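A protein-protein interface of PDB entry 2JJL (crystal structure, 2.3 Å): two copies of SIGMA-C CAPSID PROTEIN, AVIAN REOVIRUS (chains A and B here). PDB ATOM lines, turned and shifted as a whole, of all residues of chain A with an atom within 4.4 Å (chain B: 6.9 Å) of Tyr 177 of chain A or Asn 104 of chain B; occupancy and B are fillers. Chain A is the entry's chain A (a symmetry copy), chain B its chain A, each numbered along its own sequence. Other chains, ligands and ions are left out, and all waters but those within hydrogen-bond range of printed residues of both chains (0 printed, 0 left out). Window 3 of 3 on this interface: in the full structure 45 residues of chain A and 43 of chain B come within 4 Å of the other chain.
O of Asn 104 of chain B sits at hydrogen-bond distance from N of Met 115 of chain B (2.8 Å). NE2 of Gln 84 of chain B lies close to OD1 of Asn 104 of chain B (3.3 Å). O of Phe 159 of chain A is in hydrogen-bond range of N of Gly 178 of chain A, 2.9 Å away. N of Thr 189 of chain A is in hydrogen-bond range of O of Tyr 177 of chain A (3.2 Å). N of His 106 of chain B lies within hydrogen-bond range of O of Asp 113 of chain B, at 2.8 Å.
Among the printed residues, pairs that only touch across the chains: Phe 159 of chain A with His 106 of chain B (3.7 Å), Pro 160 of chain A with His 106 of chain B (3.4 Å), Pro 160 of chain A with Met 115 of chain B (3.96 Å), Tyr 177 of chain A with Leu 82 of chain B (3.8 Å), Tyr 177 of chain A with Asn 104 of chain B (3.3 Å) and Tyr 177 of chain A with Met 115 of chain B (3.95 Å).
Of the printed residues of chain B, Phe 159 of chain A touches His 106 (3.7 Å). Printed residues of chain B within 4 Å of Pro 160 of chain A: His 106 (3.4 Å) and Met 115 (3.96 Å). Of chain B, only Leu 82, Asn 104 and Met 115 come within 4 Å of Tyr 177 of chain A. Ile 188 of chain A touches none of the printed residues of chain B. Of the printed residues of chain A, Leu 82 of chain B touches Tyr 177. Asn 104 of chain B touches one residue of chain A. Of the printed residues of chain A, His 106 of chain B touches Phe 159 (3.7 Å) and Pro 160 (3.4 Å). Printed residues of chain A within 4 Å of Met 115 of chain B: Pro 160 and Tyr 177. The nearest printed residue of chain A that does not touch His 106 of chain B is Tyr 177 of chain A (6.0 Å).
Printed residues of chain A that touch a printed residue of chain B: Phe 159, Pro 160 and Tyr 177. Of the 15 printed residues of chain B, 4 touch a printed residue of chain A. Printed residues of chain B that touch a printed residue of chain A: Leu 82, Asn 104, His 106 and Met 115. Among the printed residues, 6 pairs touch across the chains. Among the printed residues, no Asp or Glu carboxylate lies within 4 Å of a Lys or Arg side-chain nitrogen of the other chain.
No position is printed for both chains. Of the 6 pairs that touch across the chains among the printed residues, none has its exchanged pair printed and touching as well.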
ATOM      1  N   PHE A 159      19.550  14.266  28.388  1.00  0.00           N
ATOM      2  CA  PHE A 159      18.605  14.398  27.304  1.00  0.00           C
ATOM      3  C   PHE A 159      17.262  14.894  27.854  1.00  0.00           C
ATOM      4  O   PHE A 159      16.944  14.639  29.018  1.00  0.00           O
ATOM      5  CB  PHE A 159      18.453  13.029  26.585  1.00  0.00           C
ATOM      6  CG  PHE A 159      18.153  11.880  27.504  1.00  0.00           C
ATOM      7  CD1 PHE A 159      19.183  11.155  28.110  1.00  0.00           C
ATOM      8  CD2 PHE A 159      16.834  11.492  27.742  1.00  0.00           C
ATOM      9  CE1 PHE A 159      18.888  10.078  28.932  1.00  0.00           C
ATOM     10  CE2 PHE A 159      16.545  10.411  28.567  1.00  0.00           C
ATOM     11  CZ  PHE A 159      17.573   9.719  29.174  1.00  0.00           C
ATOM     12  N   PRO A 160      16.477  15.604  27.021  1.00  0.00           N
ATOM     13  CA  PRO A 160      15.204  16.196  27.472  1.00  0.00           C
ATOM     14  C   PRO A 160      14.116  15.149  27.756  1.00  0.00           C
ATOM     15  O   PRO A 160      13.984  14.161  27.026  1.00  0.00           O
ATOM     16  CB  PRO A 160      14.760  17.107  26.297  1.00  0.00           C
ATOM     17  CG  PRO A 160      15.805  16.954  25.185  1.00  0.00           C
ATOM     18  CD  PRO A 160      16.775  15.856  25.590  1.00  0.00           C
ATOM     19  N   VAL A 161      13.350  15.372  28.818  1.00  0.00           N
ATOM     20  CA  VAL A 161      12.249  14.485  29.190  1.00  0.00           C
ATOM     21  C   VAL A 161      11.061  15.354  29.573  1.00  0.00           C
ATOM     22  O   VAL A 161      11.224  16.209  30.419  1.00  0.00           O
ATOM     23  CB  VAL A 161      12.657  13.662  30.447  1.00  0.00           C
ATOM     24  CG1 VAL A 161      11.521  12.753  30.895  1.00  0.00           C
ATOM     25  CG2 VAL A 161      13.965  12.847  30.174  1.00  0.00           C
ATOM     26  N   GLN A 175       9.466  20.587  31.649  1.00  0.00           N
ATOM     27  CA  GLN A 175      10.523  20.118  30.757  1.00  0.00           C
ATOM     28  C   GLN A 175      11.711  19.759  31.666  1.00  0.00           C
ATOM     29  O   GLN A 175      12.238  20.629  32.323  1.00  0.00           O
ATOM     30  CB  GLN A 175      10.849  21.254  29.778  1.00  0.00           C
ATOM     31  CG  GLN A 175      12.233  21.237  29.141  1.00  0.00           C
ATOM     32  CD  GLN A 175      12.484  19.952  28.456  1.00  0.00           C
ATOM     33  OE1 GLN A 175      11.680  19.521  27.631  1.00  0.00           O
ATOM     34  NE2 GLN A 175      13.586  19.286  28.820  1.00  0.00           N
ATOM     35  N   ALA A 176      12.084  18.473  31.751  1.00  0.00           N
ATOM     36  CA  ALA A 176      13.144  17.997  32.671  1.00  0.00           C
ATOM     37  C   ALA A 176      14.268  17.291  31.904  1.00  0.00           C
ATOM     38  O   ALA A 176      14.335  17.370  30.695  1.00  0.00           O
ATOM     39  CB  ALA A 176      12.542  17.029  33.718  1.00  0.00           C
ATOM     40  N   TYR A 177      15.112  16.530  32.592  1.00  0.00           N
ATOM     41  CA  TYR A 177      16.230  15.894  31.920  1.00  0.00           C
ATOM     42  C   TYR A 177      16.491  14.546  32.525  1.00  0.00           C
ATOM     43  O   TYR A 177      16.256  14.330  33.702  1.00  0.00           O
ATOM     44  CB  TYR A 177      17.502  16.792  31.958  1.00  0.00           C
ATOM     45  CG  TYR A 177      17.322  18.032  31.093  1.00  0.00           C
ATOM     46  CD1 TYR A 177      17.631  18.012  29.724  1.00  0.00           C
ATOM     47  CD2 TYR A 177      16.793  19.197  31.627  1.00  0.00           C
ATOM     48  CE1 TYR A 177      17.432  19.148  28.929  1.00  0.00           C
ATOM     49  CE2 TYR A 177      16.565  20.325  30.845  1.00  0.00           C
ATOM     50  CZ  TYR A 177      16.887  20.285  29.489  1.00  0.00           C
ATOM     51  OH  TYR A 177      16.669  21.404  28.709  1.00  0.00           O
ATOM     52  N   GLY A 178      16.947  13.624  31.686  1.00  0.00           N
ATOM     53  CA  GLY A 178      17.421  12.357  32.168  1.00  0.00           C
ATOM     54  C   GLY A 178      18.893  12.221  31.841  1.00  0.00           C
ATOM     55  O   GLY A 178      19.448  12.985  31.023  1.00  0.00           O
ATOM     56  N   THR A 187      18.196   7.903  34.914  1.00  0.00           N
ATOM     57  CA  THR A 187      17.473   8.576  35.973  1.00  0.00           C
ATOM     58  C   THR A 187      16.975   9.925  35.435  1.00  0.00           C
ATOM     59  O   THR A 187      17.723  10.667  34.782  1.00  0.00           O
ATOM     60  CB  THR A 187      18.403   8.801  37.192  1.00  0.00           C
ATOM     61  OG1 THR A 187      18.814   7.519  37.695  1.00  0.00           O
ATOM     62  CG2 THR A 187      17.691   9.556  38.300  1.00  0.00           C
ATOM     63  N   ILE A 188      15.716  10.221  35.699  1.00  0.00           N
ATOM     64  CA  ILE A 188      15.178  11.560  35.445  1.00  0.00           C
ATOM     65  C   ILE A 188      15.070  12.374  36.757  1.00  0.00           C
ATOM     66  O   ILE A 188      14.888  11.816  37.830  1.00  0.00           O
ATOM     67  CB  ILE A 188      13.830  11.493  34.663  1.00  0.00           C
ATOM     68  CG1 ILE A 188      12.664  11.057  35.550  1.00  0.00           C
ATOM     69  CG2 ILE A 188      13.968  10.507  33.468  1.00  0.00           C
ATOM     70  CD1 ILE A 188      11.313  10.817  34.750  1.00  0.00           C
ATOM     71  N   THR A 189      15.201  13.689  36.659  1.00  0.00           N
ATOM     72  CA  THR A 189      15.168  14.576  37.817  1.00  0.00           C
ATOM     73  C   THR A 189      14.068  15.609  37.520  1.00  0.00           C
ATOM     74  O   THR A 189      14.045  16.195  36.449  1.00  0.00           O
ATOM     75  CB  THR A 189      16.537  15.291  37.966  1.00  0.00           C
ATOM     76  OG1 THR A 189      17.555  14.305  38.174  1.00  0.00           O
ATOM     77  CG2 THR A 189      16.541  16.327  39.112  1.00  0.00           C
ATOM     78  N   LEU B  82      24.799  18.271  25.572  1.00  0.00           N
ATOM     79  CA  LEU B  82      23.745  19.184  25.976  1.00  0.00           C
ATOM     80  C   LEU B  82      24.404  20.540  26.272  1.00  0.00           C
ATOM     81  O   LEU B  82      25.017  20.733  27.323  1.00  0.00           O
ATOM     82  CB  LEU B  82      22.974  18.651  27.207  1.00  0.00           C
ATOM     83  CG  LEU B  82      21.772  19.542  27.609  1.00  0.00           C
ATOM     84  CD1 LEU B  82      20.640  19.436  26.618  1.00  0.00           C
ATOM     85  CD2 LEU B  82      21.279  19.206  29.007  1.00  0.00           C
ATOM     86  N   MET B  83      24.322  21.463  25.325  1.00  0.00           N
ATOM     87  CA  MET B  83      24.934  22.773  25.509  1.00  0.00           C
ATOM     88  C   MET B  83      23.967  23.722  26.218  1.00  0.00           C
ATOM     89  O   MET B  83      22.748  23.681  25.980  1.00  0.00           O
ATOM     90  CB  MET B  83      25.290  23.368  24.161  1.00  0.00           C
ATOM     91  CG  MET B  83      26.312  22.608  23.309  1.00  0.00           C
ATOM     92  SD  MET B  83      26.261  23.345  21.634  1.00  0.00           S
ATOM     93  CE  MET B  83      27.439  22.285  20.811  1.00  0.00           C
ATOM     94  N   GLN B  84      24.506  24.609  27.044  1.00  0.00           N
ATOM     95  CA  GLN B  84      23.720  25.609  27.762  1.00  0.00           C
ATOM     96  C   GLN B  84      24.389  26.962  27.572  1.00  0.00           C
ATOM     97  O   GLN B  84      25.544  27.128  27.896  1.00  0.00           O
ATOM     98  CB  GLN B  84      23.656  25.298  29.268  1.00  0.00           C
ATOM     99  CG  GLN B  84      23.455  23.810  29.618  1.00  0.00           C
ATOM    100  CD  GLN B  84      23.097  23.568  31.092  1.00  0.00           C
ATOM    101  OE1 GLN B  84      23.727  22.752  31.771  1.00  0.00           O
ATOM    102  NE2 GLN B  84      22.083  24.279  31.584  1.00  0.00           N
ATOM    103  N   PHE B  85      23.656  27.931  27.039  1.00  0.00           N
ATOM    104  CA  PHE B  85      24.214  29.238  26.760  1.00  0.00           C
ATOM    105  C   PHE B  85      23.073  30.242  26.778  1.00  0.00           C
ATOM    106  O   PHE B  85      21.904  29.865  26.893  1.00  0.00           O
ATOM    107  CB  PHE B  85      25.018  29.262  25.422  1.00  0.00           C
ATOM    108  CG  PHE B  85      24.260  28.699  24.214  1.00  0.00           C
ATOM    109  CD1 PHE B  85      23.444  29.518  23.436  1.00  0.00           C
ATOM    110  CD2 PHE B  85      24.388  27.368  23.857  1.00  0.00           C
ATOM    111  CE1 PHE B  85      22.768  29.029  22.319  1.00  0.00           C
ATOM    112  CE2 PHE B  85      23.732  26.861  22.719  1.00  0.00           C
ATOM    113  CZ  PHE B  85      22.910  27.683  21.962  1.00  0.00           C
ATOM    114  N   THR B 102      17.648  31.795  27.667  1.00  0.00           N
ATOM    115  CA  THR B 102      18.488  30.721  28.211  1.00  0.00           C
ATOM    116  C   THR B 102      18.184  29.522  27.324  1.00  0.00           C
ATOM    117  O   THR B 102      17.024  29.128  27.216  1.00  0.00           O
ATOM    118  CB  THR B 102      18.102  30.438  29.673  1.00  0.00           C
ATOM    119  OG1 THR B 102      18.458  31.575  30.458  1.00  0.00           O
ATOM    120  CG2 THR B 102      18.800  29.190  30.230  1.00  0.00           C
ATOM    121  N   VAL B 103      19.228  28.972  26.693  1.00  0.00           N
ATOM    122  CA  VAL B 103      19.109  27.946  25.682  1.00  0.00           C
ATOM    123  C   VAL B 103      19.790  26.670  26.126  1.00  0.00           C
ATOM    124  O   VAL B 103      20.930  26.711  26.580  1.00  0.00           O
ATOM    125  CB  VAL B 103      19.690  28.410  24.306  1.00  0.00           C
ATOM    126  CG1 VAL B 103      19.466  27.367  23.237  1.00  0.00           C
ATOM    127  CG2 VAL B 103      19.000  29.668  23.858  1.00  0.00           C
ATOM    128  N   ASN B 104      19.051  25.555  26.051  1.00  0.00           N
ATOM    129  CA  ASN B 104      19.623  24.199  26.090  1.00  0.00           C
ATOM    130  C   ASN B 104      19.534  23.656  24.672  1.00  0.00           C
ATOM    131  O   ASN B 104      18.451  23.647  24.064  1.00  0.00           O
ATOM    132  CB  ASN B 104      18.880  23.290  27.089  1.00  0.00           C
ATOM    133  CG  ASN B 104      19.286  23.602  28.558  1.00  0.00           C
ATOM    134  OD1 ASN B 104      20.323  23.170  29.030  1.00  0.00           O
ATOM    135  ND2 ASN B 104      18.509  24.411  29.218  1.00  0.00           N
ATOM    136  N   ALA B 105      20.677  23.271  24.120  1.00  0.00           N
ATOM    137  CA  ALA B 105      20.701  22.692  22.791  1.00  0.00           C
ATOM    138  C   ALA B 105      21.144  21.265  22.973  1.00  0.00           C
ATOM    139  O   ALA B 105      22.243  21.012  23.447  1.00  0.00           O
ATOM    140  CB  ALA B 105      21.655  23.448  21.902  1.00  0.00           C
ATOM    141  N   HIS B 106      20.261  20.325  22.679  1.00  0.00           N
ATOM    142  CA  HIS B 106      20.604  18.908  22.793  1.00  0.00           C
ATOM    143  C   HIS B 106      21.037  18.389  21.426  1.00  0.00           C
ATOM    144  O   HIS B 106      20.220  18.300  20.499  1.00  0.00           O
ATOM    145  CB  HIS B 106      19.422  18.086  23.338  1.00  0.00           C
ATOM    146  CG  HIS B 106      19.722  16.622  23.487  1.00  0.00           C
ATOM    147  ND1 HIS B 106      18.900  15.634  22.987  1.00  0.00           N
ATOM    148  CD2 HIS B 106      20.747  15.980  24.105  1.00  0.00           C
ATOM    149  CE1 HIS B 106      19.405  14.447  23.290  1.00  0.00           C
ATOM    150  NE2 HIS B 106      20.530  14.632  23.963  1.00  0.00           N
ATOM    151  N   THR B 112      20.024  18.795  16.203  1.00  0.00           N
ATOM    152  CA  THR B 112      20.143  19.704  17.343  1.00  0.00           C
ATOM    153  C   THR B 112      18.756  20.215  17.719  1.00  0.00           C
ATOM    154  O   THR B 112      18.094  20.865  16.915  1.00  0.00           O
ATOM    155  CB  THR B 112      21.122  20.890  17.034  1.00  0.00           C
ATOM    156  OG1 THR B 112      22.439  20.346  16.851  1.00  0.00           O
ATOM    157  CG2 THR B 112      21.125  21.943  18.184  1.00  0.00           C
ATOM    158  N   ASP B 113      18.342  19.891  18.939  1.00  0.00           N
ATOM    159  CA  ASP B 113      17.034  20.265  19.483  1.00  0.00           C
ATOM    160  C   ASP B 113      17.187  21.412  20.470  1.00  0.00           C
ATOM    161  O   ASP B 113      17.930  21.293  21.444  1.00  0.00           O
ATOM    162  CB  ASP B 113      16.402  19.031  20.171  1.00  0.00           C
ATOM    163  CG  ASP B 113      16.074  17.930  19.179  1.00  0.00           C
ATOM    164  OD1 ASP B 113      15.549  18.321  18.114  1.00  0.00           O
ATOM    165  OD2 ASP B 113      16.301  16.690  19.430  1.00  0.00           O
ATOM    166  N   TYR B 114      16.475  22.514  20.238  1.00  0.00           N
ATOM    167  CA  TYR B 114      16.575  23.666  21.111  1.00  0.00           C
ATOM    168  C   TYR B 114      15.425  23.762  22.107  1.00  0.00           C
ATOM    169  O   TYR B 114      14.255  23.696  21.706  1.00  0.00           O
ATOM    170  CB  TYR B 114      16.518  24.956  20.283  1.00  0.00           C
ATOM    171  CG  TYR B 114      17.736  25.313  19.459  1.00  0.00           C
ATOM    172  CD1 TYR B 114      19.010  25.382  20.030  1.00  0.00           C
ATOM    173  CD2 TYR B 114      17.585  25.699  18.113  1.00  0.00           C
ATOM    174  CE1 TYR B 114      20.124  25.762  19.266  1.00  0.00           C
ATOM    175  CE2 TYR B 114      18.678  26.098  17.344  1.00  0.00           C
ATOM    176  CZ  TYR B 114      19.938  26.130  17.925  1.00  0.00           C
ATOM    177  OH  TYR B 114      20.991  26.534  17.146  1.00  0.00           O
ATOM    178  N   MET B 115      15.758  23.986  23.382  1.00  0.00           N
ATOM    179  CA  MET B 115      14.764  24.313  24.396  1.00  0.00           C
ATOM    180  C   MET B 115      15.178  25.665  24.966  1.00  0.00           C
ATOM    181  O   MET B 115      16.224  25.775  25.597  1.00  0.00           O
ATOM    182  CB  MET B 115      14.688  23.255  25.529  1.00  0.00           C
ATOM    183  CG  MET B 115      14.264  21.728  25.194  1.00  0.00           C
ATOM    184  SD  MET B 115      15.268  20.711  24.044  1.00  0.00           S
ATOM    185  CE  MET B 115      16.900  20.781  24.812  1.00  0.00           C
ATOM    186  N   MET B 116      14.375  26.704  24.743  1.00  0.00           N
ATOM    187  CA  MET B 116      14.763  28.068  25.194  1.00  0.00           C
ATOM    188  C   MET B 116      13.719  28.629  26.113  1.00  0.00           C
ATOM    189  O   MET B 116      12.522  28.399  25.896  1.00  0.00           O
ATOM    190  CB  MET B 116      14.837  29.049  24.019  1.00  0.00           C
ATOM    191  CG  MET B 116      15.550  28.513  22.772  1.00  0.00           C
ATOM    192  SD  MET B 116      15.742  29.874  21.625  1.00  0.00           S
ATOM    193  CE  MET B 116      16.502  28.989  20.281  1.00  0.00           C
ATOM    194  N   SER B 117      14.156  29.397  27.117  1.00  0.00           N
ATOM    195  CA  SER B 117      13.224  30.184  27.927  1.00  0.00           C
ATOM    196  C   SER B 117      13.795  31.567  28.222  1.00  0.00           C
ATOM    197  O   SER B 117      14.995  31.713  28.372  1.00  0.00           O
ATOM    198  CB  SER B 117      12.801  29.427  29.186  1.00  0.00           C
ATOM    199  OG  SER B 117      13.903  29.222  30.010  1.00  0.00           O
